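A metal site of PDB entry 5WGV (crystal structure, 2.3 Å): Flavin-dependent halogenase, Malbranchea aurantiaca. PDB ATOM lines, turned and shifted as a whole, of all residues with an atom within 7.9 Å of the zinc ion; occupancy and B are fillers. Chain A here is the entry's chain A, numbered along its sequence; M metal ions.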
ATOM      1  N   SER A 302      11.931   8.616  -1.695  1.00  0.00           N
ATOM      2  CA  SER A 302      11.600   9.947  -2.161  1.00  0.00           C
ATOM      3  C   SER A 302      10.449   9.905  -3.156  1.00  0.00           C
ATOM      4  O   SER A 302      10.117   8.855  -3.720  1.00  0.00           O
ATOM      5  CB  SER A 302      12.819  10.626  -2.800  1.00  0.00           C
ATOM      6  OG  SER A 302      13.229   9.915  -3.960  1.00  0.00           O
ATOM      7  N   GLU A 304      10.149  10.892  -6.213  1.00  0.00           N
ATOM      8  CA  GLU A 304      10.502  10.356  -7.521  1.00  0.00           C
ATOM      9  C   GLU A 304      10.721   8.849  -7.460  1.00  0.00           C
ATOM     10  O   GLU A 304      10.382   8.133  -8.413  1.00  0.00           O
ATOM     11  CB  GLU A 304      11.749  11.066  -8.069  1.00  0.00           C
ATOM     12  CG  GLU A 304      11.548  12.565  -8.314  1.00  0.00           C
ATOM     13  CD  GLU A 304      12.834  13.274  -8.756  1.00  0.00           C
ATOM     14  OE1 GLU A 304      13.841  12.586  -9.021  1.00  0.00           O
ATOM     15  OE2 GLU A 304      12.821  14.526  -8.850  1.00  0.00           O
ATOM     16  N   TRP A 316       7.149  18.866 -11.386  1.00  0.00           N
ATOM     17  CA  TRP A 316       7.003  20.104 -10.629  1.00  0.00           C
ATOM     18  C   TRP A 316       6.325  21.154 -11.496  1.00  0.00           C
ATOM     19  O   TRP A 316       6.733  21.371 -12.646  1.00  0.00           O
ATOM     20  CB  TRP A 316       8.361  20.617 -10.146  1.00  0.00           C
ATOM     21  CG  TRP A 316       8.847  19.893  -8.943  1.00  0.00           C
ATOM     22  CD1 TRP A 316       9.789  18.906  -8.913  1.00  0.00           C
ATOM     23  CD2 TRP A 316       8.417  20.086  -7.596  1.00  0.00           C
ATOM     24  NE1 TRP A 316       9.965  18.475  -7.621  1.00  0.00           N
ATOM     25  CE2 TRP A 316       9.141  19.177  -6.799  1.00  0.00           C
ATOM     26  CE3 TRP A 316       7.483  20.935  -6.984  1.00  0.00           C
ATOM     27  CZ2 TRP A 316       8.966  19.098  -5.411  1.00  0.00           C
ATOM     28  CZ3 TRP A 316       7.318  20.852  -5.616  1.00  0.00           C
ATOM     29  CH2 TRP A 316       8.050  19.939  -4.840  1.00  0.00           C
ATOM     30  N   ARG A 595      15.711  25.178   2.453  1.00  0.00           N
ATOM     31  CA  ARG A 595      16.771  25.269   1.459  1.00  0.00           C
ATOM     32  C   ARG A 595      16.338  24.505   0.220  1.00  0.00           C
ATOM     33  O   ARG A 595      15.511  23.590   0.308  1.00  0.00           O
ATOM     34  CB  ARG A 595      18.108  24.694   1.982  1.00  0.00           C
ATOM     35  CG  ARG A 595      18.183  23.174   1.921  1.00  0.00           C
ATOM     36  CD  ARG A 595      19.607  22.644   2.002  1.00  0.00           C
ATOM     37  NE  ARG A 595      19.622  21.179   1.934  1.00  0.00           N
ATOM     38  CZ  ARG A 595      19.975  20.477   0.851  1.00  0.00           C
ATOM     39  NH1 ARG A 595      20.363  21.105  -0.255  1.00  0.00           N
ATOM     40  NH2 ARG A 595      19.944  19.150   0.896  1.00  0.00           N
ATOM     41  N   GLN A 596      16.884  24.887  -0.924  1.00  0.00           N
ATOM     42  CA  GLN A 596      16.536  24.256  -2.200  1.00  0.00           C
ATOM     43  C   GLN A 596      17.519  23.144  -2.507  1.00  0.00           C
ATOM     44  O   GLN A 596      18.734  23.325  -2.359  1.00  0.00           O
ATOM     45  CB  GLN A 596      16.533  25.301  -3.316  1.00  0.00           C
ATOM     46  CG  GLN A 596      15.293  25.290  -4.193  1.00  0.00           C
ATOM     47  CD  GLN A 596      15.383  26.300  -5.335  1.00  0.00           C
ATOM     48  OE1 GLN A 596      16.197  27.221  -5.301  1.00  0.00           O
ATOM     49  NE2 GLN A 596      14.553  26.118  -6.359  1.00  0.00           N
ATOM     50  N   CYS A 597      17.009  21.990  -2.937  1.00  0.00           N
ATOM     51  CA  CYS A 597      17.875  20.887  -3.338  1.00  0.00           C
ATOM     52  C   CYS A 597      18.640  21.273  -4.588  1.00  0.00           C
ATOM     53  O   CYS A 597      18.062  21.681  -5.594  1.00  0.00           O
ATOM     54  CB  CYS A 597      17.048  19.622  -3.602  1.00  0.00           C
ATOM     55  SG  CYS A 597      18.023  18.199  -4.162  1.00  0.00           S
ATOM     56  N   SER A 598      19.979  21.140  -4.525  1.00  0.00           N
ATOM     57  CA  SER A 598      20.808  21.467  -5.676  1.00  0.00           C
ATOM     58  C   SER A 598      20.524  20.563  -6.863  1.00  0.00           C
ATOM     59  O   SER A 598      20.827  20.928  -8.008  1.00  0.00           O
ATOM     60  CB  SER A 598      22.287  21.394  -5.288  1.00  0.00           C
ATOM     61  OG  SER A 598      22.535  20.282  -4.443  1.00  0.00           O
ATOM     62  N   GLY A 599      19.934  19.391  -6.620  1.00  0.00           N
ATOM     63  CA  GLY A 599      19.685  18.412  -7.653  1.00  0.00           C
ATOM     64  C   GLY A 599      18.399  18.609  -8.435  1.00  0.00           C
ATOM     65  O   GLY A 599      18.434  18.659  -9.671  1.00  0.00           O
ATOM     66  N   CYS A 600      17.265  18.744  -7.735  1.00  0.00           N
ATOM     67  CA  CYS A 600      15.971  18.816  -8.388  1.00  0.00           C
ATOM     68  C   CYS A 600      15.243  20.141  -8.206  1.00  0.00           C
ATOM     69  O   CYS A 600      14.197  20.341  -8.836  1.00  0.00           O
ATOM     70  CB  CYS A 600      15.056  17.679  -7.881  1.00  0.00           C
ATOM     71  SG  CYS A 600      14.611  17.841  -6.141  1.00  0.00           S
ATOM     72  N   GLY A 601      15.749  21.043  -7.362  1.00  0.00           N
ATOM     73  CA  GLY A 601      15.083  22.313  -7.132  1.00  0.00           C
ATOM     74  C   GLY A 601      13.994  22.300  -6.086  1.00  0.00           C
ATOM     75  O   GLY A 601      13.410  23.356  -5.814  1.00  0.00           O
ATOM     76  N   ALA A 602      13.696  21.146  -5.488  1.00  0.00           N
ATOM     77  CA  ALA A 602      12.625  21.087  -4.510  1.00  0.00           C
ATOM     78  C   ALA A 602      13.063  21.727  -3.190  1.00  0.00           C
ATOM     79  O   ALA A 602      14.218  21.630  -2.784  1.00  0.00           O
ATOM     80  CB  ALA A 602      12.202  19.645  -4.257  1.00  0.00           C
ATOM     81  N   TRP A 603      12.117  22.372  -2.527  1.00  0.00           N
ATOM     82  CA  TRP A 603      12.382  23.023  -1.257  1.00  0.00           C
ATOM     83  C   TRP A 603      12.299  22.020  -0.112  1.00  0.00           C
ATOM     84  O   TRP A 603      11.374  21.193  -0.050  1.00  0.00           O
ATOM     85  CB  TRP A 603      11.412  24.182  -1.052  1.00  0.00           C
ATOM     86  CG  TRP A 603      11.771  25.320  -1.954  1.00  0.00           C
ATOM     87  CD1 TRP A 603      11.336  25.528  -3.227  1.00  0.00           C
ATOM     88  CD2 TRP A 603      12.681  26.387  -1.656  1.00  0.00           C
ATOM     89  NE1 TRP A 603      11.896  26.683  -3.742  1.00  0.00           N
ATOM     90  CE2 TRP A 603      12.723  27.218  -2.796  1.00  0.00           C
ATOM     91  CE3 TRP A 603      13.440  26.727  -0.539  1.00  0.00           C
ATOM     92  CZ2 TRP A 603      13.511  28.366  -2.845  1.00  0.00           C
ATOM     93  CZ3 TRP A 603      14.221  27.868  -0.590  1.00  0.00           C
ATOM     94  CH2 TRP A 603      14.255  28.679  -1.735  1.00  0.00           C
ATOM     95  N   LEU A 604      13.284  22.081   0.785  1.00  0.00           N
ATOM     96  CA  LEU A 604      13.454  21.110   1.852  1.00  0.00           C
ATOM     97  C   LEU A 604      13.428  21.802   3.208  1.00  0.00           C
ATOM     98  O   LEU A 604      13.854  22.946   3.340  1.00  0.00           O
ATOM     99  CB  LEU A 604      14.794  20.361   1.708  1.00  0.00           C
ATOM    100  CG  LEU A 604      15.107  19.712   0.363  1.00  0.00           C
ATOM    101  CD1 LEU A 604      16.523  19.129   0.351  1.00  0.00           C
ATOM    102  CD2 LEU A 604      14.078  18.648   0.041  1.00  0.00           C
ATOM    103  N   LYS A 612      18.723  13.704   3.417  1.00  0.00           N
ATOM    104  CA  LYS A 612      18.478  13.543   1.996  1.00  0.00           C
ATOM    105  C   LYS A 612      17.261  14.354   1.562  1.00  0.00           C
ATOM    106  O   LYS A 612      16.348  14.628   2.345  1.00  0.00           O
ATOM    107  CB  LYS A 612      18.269  12.074   1.624  1.00  0.00           C
ATOM    108  CG  LYS A 612      16.895  11.534   1.994  1.00  0.00           C
ATOM    109  CD  LYS A 612      16.643  10.152   1.408  1.00  0.00           C
ATOM    110  CE  LYS A 612      15.178   9.764   1.540  1.00  0.00           C
ATOM    111  NZ  LYS A 612      14.909   8.387   1.045  1.00  0.00           N
ATOM    112  N   CYS A 613      17.259  14.738   0.282  1.00  0.00           N
ATOM    113  CA  CYS A 613      16.073  15.322  -0.324  1.00  0.00           C
ATOM    114  C   CYS A 613      14.924  14.322  -0.279  1.00  0.00           C
ATOM    115  O   CYS A 613      15.078  13.155  -0.654  1.00  0.00           O
ATOM    116  CB  CYS A 613      16.389  15.723  -1.768  1.00  0.00           C
ATOM    117  SG  CYS A 613      15.050  16.529  -2.668  1.00  0.00           S
ATOM    118  N   HIS A 614      13.767  14.762   0.229  1.00  0.00           N
ATOM    119  CA  HIS A 614      12.591  13.898   0.285  1.00  0.00           C
ATOM    120  C   HIS A 614      11.891  13.766  -1.062  1.00  0.00           C
ATOM    121  O   HIS A 614      10.973  12.948  -1.192  1.00  0.00           O
ATOM    122  CB  HIS A 614      11.588  14.422   1.329  1.00  0.00           C
ATOM    123  CG  HIS A 614      11.037  15.772   1.004  1.00  0.00           C
ATOM    124  ND1 HIS A 614       9.932  15.959   0.191  1.00  0.00           N
ATOM    125  CD2 HIS A 614      11.439  17.010   1.366  1.00  0.00           C
ATOM    126  CE1 HIS A 614       9.683  17.243   0.064  1.00  0.00           C
ATOM    127  NE2 HIS A 614      10.580  17.915   0.768  1.00  0.00           N
ATOM    128  N   SER A 615      12.299  14.563  -2.042  1.00  0.00           N
ATOM    129  CA  SER A 615      11.663  14.593  -3.352  1.00  0.00           C
ATOM    130  C   SER A 615      12.417  13.777  -4.388  1.00  0.00           C
ATOM    131  O   SER A 615      11.792  13.075  -5.188  1.00  0.00           O
ATOM    132  CB  SER A 615      11.527  16.046  -3.823  1.00  0.00           C
ATOM    133  OG  SER A 615      10.654  16.143  -4.933  1.00  0.00           O
ATOM    134  N   CYS A 616      13.748  13.845  -4.391  1.00  0.00           N
ATOM    135  CA  CYS A 616      14.548  13.062  -5.313  1.00  0.00           C
ATOM    136  C   CYS A 616      15.554  12.147  -4.627  1.00  0.00           C
ATOM    137  O   CYS A 616      16.168  11.326  -5.302  1.00  0.00           O
ATOM    138  CB  CYS A 616      15.305  13.985  -6.279  1.00  0.00           C
ATOM    139  SG  CYS A 616      16.807  14.707  -5.607  1.00  0.00           S
ATOM    140  N   GLY A 617      15.751  12.275  -3.320  1.00  0.00           N
ATOM    141  CA  GLY A 617      16.626  11.375  -2.606  1.00  0.00           C
ATOM    142  C   GLY A 617      18.097  11.744  -2.597  1.00  0.00           C
ATOM    143  O   GLY A 617      18.898  10.978  -2.041  1.00  0.00           O
ATOM    144  N   LEU A 618      18.484  12.869  -3.180  1.00  0.00           N
ATOM    145  CA  LEU A 618      19.894  13.239  -3.199  1.00  0.00           C
ATOM    146  C   LEU A 618      20.354  13.691  -1.810  1.00  0.00           C
ATOM    147  O   LEU A 618      19.660  14.439  -1.107  1.00  0.00           O
ATOM    148  CB  LEU A 618      20.135  14.347  -4.222  1.00  0.00           C
ATOM    149  CG  LEU A 618      21.468  15.099  -4.148  1.00  0.00           C
ATOM    150  CD1 LEU A 618      22.654  14.181  -4.425  1.00  0.00           C
ATOM    151  CD2 LEU A 618      21.457  16.273  -5.107  1.00  0.00           C
ATOM    152  N   LEU A 619      21.544  13.237  -1.425  1.00  0.00           N
ATOM    153  CA  LEU A 619      22.142  13.635  -0.163  1.00  0.00           C
ATOM    154  C   LEU A 619      22.718  15.040  -0.261  1.00  0.00           C
ATOM    155  O   LEU A 619      23.524  15.338  -1.144  1.00  0.00           O
ATOM    156  CB  LEU A 619      23.246  12.657   0.226  1.00  0.00           C
ATOM    157  CG  LEU A 619      22.976  11.612   1.299  1.00  0.00           C
ATOM    158  CD1 LEU A 619      24.290  11.054   1.853  1.00  0.00           C
ATOM    159  CD2 LEU A 619      22.117  12.177   2.429  1.00  0.00           C
HETATM  160 ZN    ZN M   1      16.169  16.746  -4.737  1.00  0.00          ZN
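N of Leu 618 lies close to SG of Cys 616 (3.5 Å).
O of Leu 618 is in hydrogen-bond range of N of Cys 613, at 2.8 Å.
The side-chain sulfur (SG) of Cys 613 sits close to the backbone NH (N) of Ser 615, 3.4 Å away.
SG of Cys 600 sits close to N of Ala 602, at 3.5 Å.
SG of Cys 597 sits close to N of Gly 599 (3.3 Å).
N of Cys 597 lies within hydrogen-bond range of O of Ala 602, at 2.8 Å.
Of the 21 residues printed, 4 come within 4 Å of the zinc ion.
The nearest printed residue that does not touch the zinc ion is Leu 618 (4.7 Å).
The zinc ion is bound by SG of Cys 616, at 2.3 Å.
The zinc ion is bound by SG of Cys 613, at 2.4 Å.
The zinc ion is bound by SG of Cys 600 (2.4 Å).
SG of Cys 597 is bound to the zinc ion, 2.4 Å away.
The zinc ion has four donor atoms within binding distance.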
